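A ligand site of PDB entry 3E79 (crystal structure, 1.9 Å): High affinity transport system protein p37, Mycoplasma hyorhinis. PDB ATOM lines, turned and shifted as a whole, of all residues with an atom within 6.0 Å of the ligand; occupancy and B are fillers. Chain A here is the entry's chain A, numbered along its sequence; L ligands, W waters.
The side-chain hydroxyl (OG) of Ser 255 lies within hydrogen-bond range of the backbone NH (N) of Lys 258.
The backbone carbonyl oxygen (O) of Ile 341 sits at hydrogen-bond distance from the backbone NH (N) of Tyr 215, 2.9 Å away.
NZ of Lys 258 sits at hydrogen-bond distance from OG of Ser 257 (3.3 Å).
NZ of Lys 258 is in salt-bridge range of OE1 of Glu 308, 2.7 Å away.
OD2 of Asp 344 is in hydrogen-bond range of OH of Tyr 381, 2.6 Å away.
The backbone carbonyl oxygen (O) of Pro 377 is in hydrogen-bond range of the side-chain amide nitrogen (ND2) of Asn 200, at 2.9 Å.
The backbone carbonyl oxygen (O) of Gly 380 sits at hydrogen-bond distance from the side-chain hydroxyl (OG1) of Thr 149, at 2.6 Å.
An oxygen (O7) of the ligand sits at hydrogen-bond distance from the side-chain hydroxyl (OG) of Ser 255, 2.6 Å away.
O5 of the ligand sits at hydrogen-bond distance from OH of Tyr 215, 2.6 Å away.
The backbone NH (N) of Ser 257 sits at hydrogen-bond distance from an oxygen (O5) of the ligand, at 2.9 Å.
An oxygen (O5) of the ligand is in hydrogen-bond range of the side-chain hydroxyl (OG) of Ser 257, 2.7 Å away.
NZ of Lys 258 is in salt-bridge range of O2 of the ligand.
An oxygen (O6) of the ligand is in hydrogen-bond range of the backbone NH of Ser 256 (2.8 Å).
OH of Tyr 343 lies close to S1 of the ligand (3.5 Å).
NZ of Lys 129 lies within salt-bridge range of O6 of the ligand (3.2 Å).
Water W2 lies within hydrogen-bond range of OG of Ser 256 (2.7 Å), O6 of the ligand (2.7 Å), N of Lys 129 (3.0 Å) and N of Gly 128 (3.3 Å).
Water W5 bridges N1 of the ligand (2.7 Å) and OH of Tyr 206 (2.8 Å).
Water W1 lies within hydrogen-bond range of O3 of the ligand (2.8 Å) and NZ of Lys 129 (2.8 Å).
Water W4 bridges an oxygen (O7) of the ligand and the side-chain amino group (NZ) of Lys 129.
Water W6 bridges OE1 of Glu 308 and O2 of the ligand.
Water W3 bridges the side-chain carboxylate of Asp 344 and an oxygen (O3) of the ligand.
The side-chain carboxylate of Asp 344 sits close to a sulfur (S1) of the ligand (3.2 Å).
Ala 126 touches the ligand (CB to O4, 3.7 Å).
Asn 200 touches the ligand.
Val 201 touches the ligand (CG1 to C2, 3.5 Å).
Glu 308 touches the ligand.
CZ2 of Trp 314 touches C6 of the ligand (3.4 Å).
Pro 377 touches the ligand (O to C2, 3.9 Å).
O of Leu 378 touches C2 of the ligand, 3.7 Å away.
Leu 379 touches the ligand.
Gly 380 touches the ligand (CA to N1, 3.5 Å).
Hydrophobic or aromatic side chains that line the ligand: Ala 126, Val 201, Tyr 215, Trp 314 and Tyr 343.
The nearest printed residue that does not touch the ligand is Tyr 381 (4.2 Å).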
ATOM      1  N   ALA A 126      26.547  10.622  10.316  1.00  0.00           N
ATOM      2  CA  ALA A 126      26.635   9.737   9.168  1.00  0.00           C
ATOM      3  C   ALA A 126      27.513   8.528   9.481  1.00  0.00           C
ATOM      4  O   ALA A 126      28.543   8.611  10.157  1.00  0.00           O
ATOM      5  CB  ALA A 126      27.203  10.462   7.964  1.00  0.00           C
ATOM      6  N   SER A 127      27.092   7.369   8.983  1.00  0.00           N
ATOM      7  CA  SER A 127      27.797   6.149   9.388  1.00  0.00           C
ATOM      8  C   SER A 127      29.218   6.088   8.866  1.00  0.00           C
ATOM      9  O   SER A 127      30.126   5.711   9.596  1.00  0.00           O
ATOM     10  CB  SER A 127      26.993   4.933   8.928  1.00  0.00           C
ATOM     11  OG  SER A 127      26.928   4.874   7.519  1.00  0.00           O
ATOM     12  N   GLY A 128      29.464   6.420   7.595  1.00  0.00           N
ATOM     13  CA  GLY A 128      30.820   6.247   7.078  1.00  0.00           C
ATOM     14  C   GLY A 128      31.824   7.104   7.835  1.00  0.00           C
ATOM     15  O   GLY A 128      32.903   6.660   8.247  1.00  0.00           O
ATOM     16  N   LYS A 129      31.470   8.376   8.015  1.00  0.00           N
ATOM     17  CA  LYS A 129      32.344   9.265   8.802  1.00  0.00           C
ATOM     18  C   LYS A 129      32.613   8.689  10.180  1.00  0.00           C
ATOM     19  O   LYS A 129      33.714   8.777  10.755  1.00  0.00           O
ATOM     20  CB  LYS A 129      31.702  10.648   8.879  1.00  0.00           C
ATOM     21  CG  LYS A 129      31.749  11.397   7.548  1.00  0.00           C
ATOM     22  CD  LYS A 129      30.911  12.653   7.634  1.00  0.00           C
ATOM     23  CE  LYS A 129      31.110  13.580   6.443  1.00  0.00           C
ATOM     24  NZ  LYS A 129      29.820  13.834   5.763  1.00  0.00           N
ATOM     25  N   THR A 149      15.327   4.667   6.961  1.00  0.00           N
ATOM     26  CA  THR A 149      14.639   5.678   6.146  1.00  0.00           C
ATOM     27  C   THR A 149      13.604   5.006   5.260  1.00  0.00           C
ATOM     28  O   THR A 149      13.740   3.830   4.908  1.00  0.00           O
ATOM     29  CB  THR A 149      15.689   6.517   5.382  1.00  0.00           C
ATOM     30  OG1 THR A 149      15.082   7.681   4.818  1.00  0.00           O
ATOM     31  CG2 THR A 149      16.329   5.763   4.211  1.00  0.00           C
ATOM     32  N   ASN A 200       8.378  18.592   2.793  1.00  0.00           N
ATOM     33  CA  ASN A 200       9.625  17.893   3.086  1.00  0.00           C
ATOM     34  C   ASN A 200      10.167  17.097   1.909  1.00  0.00           C
ATOM     35  O   ASN A 200      11.305  17.301   1.486  1.00  0.00           O
ATOM     36  CB  ASN A 200       9.372  16.970   4.287  1.00  0.00           C
ATOM     37  CG  ASN A 200      10.647  16.455   4.930  1.00  0.00           C
ATOM     38  OD1 ASN A 200      11.667  17.140   4.925  1.00  0.00           O
ATOM     39  ND2 ASN A 200      10.588  15.245   5.473  1.00  0.00           N
ATOM     40  N   VAL A 201       9.386  16.156   1.384  1.00  0.00           N
ATOM     41  CA  VAL A 201       9.832  15.300   0.291  1.00  0.00           C
ATOM     42  C   VAL A 201       8.714  15.073  -0.727  1.00  0.00           C
ATOM     43  O   VAL A 201       7.560  15.359  -0.429  1.00  0.00           O
ATOM     44  CB  VAL A 201      10.302  13.920   0.777  1.00  0.00           C
ATOM     45  CG1 VAL A 201      11.403  14.046   1.820  1.00  0.00           C
ATOM     46  CG2 VAL A 201       9.142  13.123   1.340  1.00  0.00           C
ATOM     47  N   TYR A 206       8.544   7.220  -2.760  1.00  0.00           N
ATOM     48  CA  TYR A 206       8.898   6.447  -1.583  1.00  0.00           C
ATOM     49  C   TYR A 206       7.882   5.342  -1.306  1.00  0.00           C
ATOM     50  O   TYR A 206       6.709   5.479  -1.641  1.00  0.00           O
ATOM     51  CB  TYR A 206       8.959   7.322  -0.326  1.00  0.00           C
ATOM     52  CG  TYR A 206      10.071   8.314  -0.208  1.00  0.00           C
ATOM     53  CD1 TYR A 206       9.910   9.597  -0.742  1.00  0.00           C
ATOM     54  CD2 TYR A 206      11.262   8.017   0.425  1.00  0.00           C
ATOM     55  CE1 TYR A 206      10.906  10.533  -0.650  1.00  0.00           C
ATOM     56  CE2 TYR A 206      12.281   8.954   0.537  1.00  0.00           C
ATOM     57  CZ  TYR A 206      12.093  10.205  -0.005  1.00  0.00           C
ATOM     58  OH  TYR A 206      13.075  11.158   0.077  1.00  0.00           O
ATOM     59  N   TYR A 215      21.679   3.545   2.535  1.00  0.00           N
ATOM     60  CA  TYR A 215      21.525   4.481   1.418  1.00  0.00           C
ATOM     61  C   TYR A 215      22.693   4.251   0.456  1.00  0.00           C
ATOM     62  O   TYR A 215      23.619   3.485   0.746  1.00  0.00           O
ATOM     63  CB  TYR A 215      21.435   5.939   1.846  1.00  0.00           C
ATOM     64  CG  TYR A 215      22.711   6.615   2.299  1.00  0.00           C
ATOM     65  CD1 TYR A 215      23.423   6.096   3.379  1.00  0.00           C
ATOM     66  CD2 TYR A 215      23.213   7.749   1.675  1.00  0.00           C
ATOM     67  CE1 TYR A 215      24.592   6.689   3.817  1.00  0.00           C
ATOM     68  CE2 TYR A 215      24.391   8.359   2.092  1.00  0.00           C
ATOM     69  CZ  TYR A 215      25.058   7.818   3.174  1.00  0.00           C
ATOM     70  OH  TYR A 215      26.223   8.401   3.593  1.00  0.00           O
ATOM     71  N   ASN A 254      35.855  13.830   2.275  1.00  0.00           N
ATOM     72  CA  ASN A 254      35.476  12.917   3.356  1.00  0.00           C
ATOM     73  C   ASN A 254      34.027  12.492   3.283  1.00  0.00           C
ATOM     74  O   ASN A 254      33.504  11.850   4.192  1.00  0.00           O
ATOM     75  CB  ASN A 254      35.804  13.590   4.701  1.00  0.00           C
ATOM     76  CG  ASN A 254      35.114  14.924   4.881  1.00  0.00           C
ATOM     77  OD1 ASN A 254      34.273  15.321   4.078  1.00  0.00           O
ATOM     78  ND2 ASN A 254      35.457  15.663   5.941  1.00  0.00           N
ATOM     79  N   SER A 255      33.335  12.844   2.191  1.00  0.00           N
ATOM     80  CA  SER A 255      31.943  12.419   2.037  1.00  0.00           C
ATOM     81  C   SER A 255      31.790  10.987   1.571  1.00  0.00           C
ATOM     82  O   SER A 255      32.483  10.555   0.644  1.00  0.00           O
ATOM     83  CB  SER A 255      31.258  13.362   1.035  1.00  0.00           C
ATOM     84  OG  SER A 255      29.972  12.876   0.693  1.00  0.00           O
ATOM     85  N   SER A 256      30.890  10.176   2.142  1.00  0.00           N
ATOM     86  CA  SER A 256      30.694   8.859   1.560  1.00  0.00           C
ATOM     87  C   SER A 256      29.913   8.951   0.232  1.00  0.00           C
ATOM     88  O   SER A 256      30.395   8.493  -0.811  1.00  0.00           O
ATOM     89  CB  SER A 256      29.961   7.921   2.517  1.00  0.00           C
ATOM     90  OG  SER A 256      30.750   7.749   3.689  1.00  0.00           O
ATOM     91  N   SER A 257      28.721   9.542   0.264  1.00  0.00           N
ATOM     92  CA  SER A 257      27.823   9.490  -0.885  1.00  0.00           C
ATOM     93  C   SER A 257      28.116  10.523  -1.962  1.00  0.00           C
ATOM     94  O   SER A 257      27.515  10.420  -3.042  1.00  0.00           O
ATOM     95  CB  SER A 257      26.359   9.668  -0.438  1.00  0.00           C
ATOM     96  OG  SER A 257      26.170  10.970   0.119  1.00  0.00           O
ATOM     97  N   LYS A 258      28.979  11.488  -1.700  1.00  0.00           N
ATOM     98  CA  LYS A 258      29.380  12.448  -2.734  1.00  0.00           C
ATOM     99  C   LYS A 258      30.858  12.349  -3.055  1.00  0.00           C
ATOM    100  O   LYS A 258      31.444  13.220  -3.696  1.00  0.00           O
ATOM    101  CB  LYS A 258      28.951  13.870  -2.311  1.00  0.00           C
ATOM    102  CG  LYS A 258      27.447  14.025  -2.233  1.00  0.00           C
ATOM    103  CD  LYS A 258      27.017  15.204  -1.377  1.00  0.00           C
ATOM    104  CE  LYS A 258      27.229  14.951   0.116  1.00  0.00           C
ATOM    105  NZ  LYS A 258      26.073  14.232   0.725  1.00  0.00           N
ATOM    106  N   GLU A 308      23.975  11.977  -3.474  1.00  0.00           N
ATOM    107  CA  GLU A 308      23.312  10.856  -2.809  1.00  0.00           C
ATOM    108  C   GLU A 308      22.243  10.362  -3.784  1.00  0.00           C
ATOM    109  O   GLU A 308      21.767  11.147  -4.610  1.00  0.00           O
ATOM    110  CB  GLU A 308      22.768  11.217  -1.450  1.00  0.00           C
ATOM    111  CG  GLU A 308      22.213  12.560  -1.142  1.00  0.00           C
ATOM    112  CD  GLU A 308      23.069  13.800  -1.194  1.00  0.00           C
ATOM    113  OE1 GLU A 308      23.521  14.329  -0.154  1.00  0.00           O
ATOM    114  OE2 GLU A 308      23.283  14.325  -2.304  1.00  0.00           O
ATOM    115  N   TRP A 314      14.141  15.111  -2.178  1.00  0.00           N
ATOM    116  CA  TRP A 314      13.877  16.067  -1.102  1.00  0.00           C
ATOM    117  C   TRP A 314      14.261  17.468  -1.568  1.00  0.00           C
ATOM    118  O   TRP A 314      14.486  18.414  -0.807  1.00  0.00           O
ATOM    119  CB  TRP A 314      14.581  15.653   0.193  1.00  0.00           C
ATOM    120  CG  TRP A 314      16.066  15.528   0.074  1.00  0.00           C
ATOM    121  CD1 TRP A 314      17.011  16.517   0.074  1.00  0.00           C
ATOM    122  CD2 TRP A 314      16.764  14.279  -0.090  1.00  0.00           C
ATOM    123  NE1 TRP A 314      18.260  15.948  -0.061  1.00  0.00           N
ATOM    124  CE2 TRP A 314      18.133  14.580  -0.160  1.00  0.00           C
ATOM    125  CE3 TRP A 314      16.328  12.962  -0.159  1.00  0.00           C
ATOM    126  CZ2 TRP A 314      19.083  13.577  -0.319  1.00  0.00           C
ATOM    127  CZ3 TRP A 314      17.279  11.960  -0.309  1.00  0.00           C
ATOM    128  CH2 TRP A 314      18.633  12.278  -0.389  1.00  0.00           C
ATOM    129  N   ILE A 341      25.518   1.570   2.064  1.00  0.00           N
ATOM    130  CA  ILE A 341      26.119   1.610   3.408  1.00  0.00           C
ATOM    131  C   ILE A 341      25.025   1.973   4.402  1.00  0.00           C
ATOM    132  O   ILE A 341      23.981   2.466   3.968  1.00  0.00           O
ATOM    133  CB  ILE A 341      27.293   2.596   3.546  1.00  0.00           C
ATOM    134  CG1 ILE A 341      26.884   4.065   3.395  1.00  0.00           C
ATOM    135  CG2 ILE A 341      28.432   2.214   2.612  1.00  0.00           C
ATOM    136  CD1 ILE A 341      27.993   5.057   3.684  1.00  0.00           C
ATOM    137  N   PRO A 342      25.181   1.759   5.703  1.00  0.00           N
ATOM    138  CA  PRO A 342      24.118   2.071   6.660  1.00  0.00           C
ATOM    139  C   PRO A 342      23.716   3.540   6.760  1.00  0.00           C
ATOM    140  O   PRO A 342      24.520   4.435   6.466  1.00  0.00           O
ATOM    141  CB  PRO A 342      24.743   1.679   8.035  1.00  0.00           C
ATOM    142  CG  PRO A 342      25.784   0.674   7.655  1.00  0.00           C
ATOM    143  CD  PRO A 342      26.372   1.163   6.362  1.00  0.00           C
ATOM    144  N   TYR A 343      22.471   3.733   7.194  1.00  0.00           N
ATOM    145  CA  TYR A 343      21.916   5.051   7.453  1.00  0.00           C
ATOM    146  C   TYR A 343      22.545   5.608   8.730  1.00  0.00           C
ATOM    147  O   TYR A 343      23.454   4.976   9.283  1.00  0.00           O
ATOM    148  CB  TYR A 343      20.378   5.042   7.490  1.00  0.00           C
ATOM    149  CG  TYR A 343      19.844   6.260   6.743  1.00  0.00           C
ATOM    150  CD1 TYR A 343      19.087   7.239   7.352  1.00  0.00           C
ATOM    151  CD2 TYR A 343      20.131   6.424   5.390  1.00  0.00           C
ATOM    152  CE1 TYR A 343      18.614   8.330   6.651  1.00  0.00           C
ATOM    153  CE2 TYR A 343      19.671   7.519   4.678  1.00  0.00           C
ATOM    154  CZ  TYR A 343      18.911   8.468   5.319  1.00  0.00           C
ATOM    155  OH  TYR A 343      18.451   9.564   4.607  1.00  0.00           O
ATOM    156  N   ASP A 344      22.142   6.785   9.175  1.00  0.00           N
ATOM    157  CA  ASP A 344      22.914   7.470  10.214  1.00  0.00           C
ATOM    158  C   ASP A 344      22.831   6.740  11.553  1.00  0.00           C
ATOM    159  O   ASP A 344      21.908   5.965  11.803  1.00  0.00           O
ATOM    160  CB  ASP A 344      22.432   8.912  10.336  1.00  0.00           C
ATOM    161  CG  ASP A 344      22.779   9.802   9.156  1.00  0.00           C
ATOM    162  OD1 ASP A 344      23.436   9.319   8.212  1.00  0.00           O
ATOM    163  OD2 ASP A 344      22.397  10.988   9.150  1.00  0.00           O
ATOM    164  N   PRO A 377      11.712  12.467  10.889  1.00  0.00           N
ATOM    165  CA  PRO A 377      11.240  12.484   9.492  1.00  0.00           C
ATOM    166  C   PRO A 377      11.758  13.668   8.685  1.00  0.00           C
ATOM    167  O   PRO A 377      11.915  13.590   7.466  1.00  0.00           O
ATOM    168  CB  PRO A 377       9.721  12.539   9.655  1.00  0.00           C
ATOM    169  CG  PRO A 377       9.503  11.781  10.927  1.00  0.00           C
ATOM    170  CD  PRO A 377      10.603  12.245  11.834  1.00  0.00           C
ATOM    171  N   LEU A 378      12.042  14.781   9.367  1.00  0.00           N
ATOM    172  CA  LEU A 378      12.561  15.972   8.710  1.00  0.00           C
ATOM    173  C   LEU A 378      13.994  15.752   8.225  1.00  0.00           C
ATOM    174  O   LEU A 378      14.444  16.473   7.323  1.00  0.00           O
ATOM    175  CB  LEU A 378      12.489  17.183   9.641  1.00  0.00           C
ATOM    176  CG  LEU A 378      11.114  17.527  10.238  1.00  0.00           C
ATOM    177  CD1 LEU A 378      11.193  18.751  11.137  1.00  0.00           C
ATOM    178  CD2 LEU A 378      10.070  17.749   9.147  1.00  0.00           C
ATOM    179  N   LEU A 379      14.701  14.773   8.788  1.00  0.00           N
ATOM    180  CA  LEU A 379      16.073  14.519   8.376  1.00  0.00           C
ATOM    181  C   LEU A 379      16.168  13.289   7.496  1.00  0.00           C
ATOM    182  O   LEU A 379      17.222  12.971   6.951  1.00  0.00           O
ATOM    183  CB  LEU A 379      17.006  14.324   9.578  1.00  0.00           C
ATOM    184  CG  LEU A 379      16.884  15.369  10.698  1.00  0.00           C
ATOM    185  CD1 LEU A 379      17.981  15.185  11.737  1.00  0.00           C
ATOM    186  CD2 LEU A 379      16.905  16.772  10.116  1.00  0.00           C
ATOM    187  N   GLY A 380      15.044  12.570   7.384  1.00  0.00           N
ATOM    188  CA  GLY A 380      15.074  11.324   6.646  1.00  0.00           C
ATOM    189  C   GLY A 380      15.068  10.122   7.568  1.00  0.00           C
ATOM    190  O   GLY A 380      15.220   8.998   7.093  1.00  0.00           O
ATOM    191  N   TYR A 381      14.897  10.332   8.861  1.00  0.00           N
ATOM    192  CA  TYR A 381      14.868   9.197   9.800  1.00  0.00           C
ATOM    193  C   TYR A 381      13.436   8.795  10.096  1.00  0.00           C
ATOM    194  O   TYR A 381      12.775   9.428  10.922  1.00  0.00           O
ATOM    195  CB  TYR A 381      15.562   9.546  11.107  1.00  0.00           C
ATOM    196  CG  TYR A 381      16.909  10.191  11.030  1.00  0.00           C
ATOM    197  CD1 TYR A 381      17.837   9.832  10.057  1.00  0.00           C
ATOM    198  CD2 TYR A 381      17.269  11.191  11.947  1.00  0.00           C
ATOM    199  CE1 TYR A 381      19.086  10.435   9.984  1.00  0.00           C
ATOM    200  CE2 TYR A 381      18.513  11.787  11.884  1.00  0.00           C
ATOM    201  CZ  TYR A 381      19.410  11.409  10.902  1.00  0.00           C
ATOM    202  OH  TYR A 381      20.645  12.009  10.849  1.00  0.00           O
HETATM  203  N1  LIG L   1      15.552  12.890   3.558  1.00  0.00           N
HETATM  204  C1  LIG L   1      15.286  14.164   3.936  1.00  0.00           C
HETATM  205  C2  LIG L   1      13.852  14.586   4.251  1.00  0.00           C
HETATM  206  N2  LIG L   1      16.285  15.081   3.929  1.00  0.00           N
HETATM  207  C3  LIG L   1      17.558  14.652   3.708  1.00  0.00           C
HETATM  208  N3  LIG L   1      18.517  15.580   3.740  1.00  0.00           N
HETATM  209  C4  LIG L   1      17.861  13.339   3.340  1.00  0.00           C
HETATM  210  C5  LIG L   1      16.785  12.445   3.297  1.00  0.00           C
HETATM  211  C6  LIG L   1      19.264  12.807   3.002  1.00  0.00           C
HETATM  212  N4  LIG L   1      20.036  12.160   4.078  1.00  0.00           N
HETATM  213  C7  LIG L   1      19.738  12.386   5.362  1.00  0.00           C
HETATM  214  S1  LIG L   1      20.843  11.507   6.366  1.00  0.00           S
HETATM  215  C8  LIG L   1      21.678  10.804   5.011  1.00  0.00           C
HETATM  216  C9  LIG L   1      21.086  11.316   3.860  1.00  0.00           C
HETATM  217  C10 LIG L   1      21.613  10.872   2.475  1.00  0.00           C
HETATM  218  C11 LIG L   1      22.810   9.798   5.180  1.00  0.00           C
HETATM  219  C12 LIG L   1      24.151  10.486   5.422  1.00  0.00           C
HETATM  220  O1  LIG L   1      24.418  11.374   4.322  1.00  0.00           O
HETATM  221  P1  LIG L   1      25.397  12.621   4.459  1.00  0.00           P
HETATM  222  O2  LIG L   1      25.212  13.491   3.285  1.00  0.00           O
HETATM  223  O3  LIG L   1      25.184  13.277   5.800  1.00  0.00           O
HETATM  224  O4  LIG L   1      26.855  12.034   4.604  1.00  0.00           O
HETATM  225  P2  LIG L   1      27.817  11.669   3.410  1.00  0.00           P
HETATM  226  O5  LIG L   1      27.257  10.601   2.539  1.00  0.00           O
HETATM  227  O6  LIG L   1      29.168  11.198   4.111  1.00  0.00           O
HETATM  228  O7  LIG L   1      28.180  13.018   2.637  1.00  0.00           O
HETATM  229  O   HOH W   1      27.407  14.193   7.212  1.00  0.00           O
HETATM  230  O   HOH W   2      29.700   9.105   5.714  1.00  0.00           O
HETATM  231  O   HOH W   3      23.811  13.062   8.359  1.00  0.00           O
HETATM  232  O   HOH W   4      27.685  15.476   3.910  1.00  0.00           O
HETATM  233  O   HOH W   5      14.159  10.785   2.588  1.00  0.00           O
HETATM  234  O   HOH W   6      22.633  14.428   2.474  1.00  0.00           O
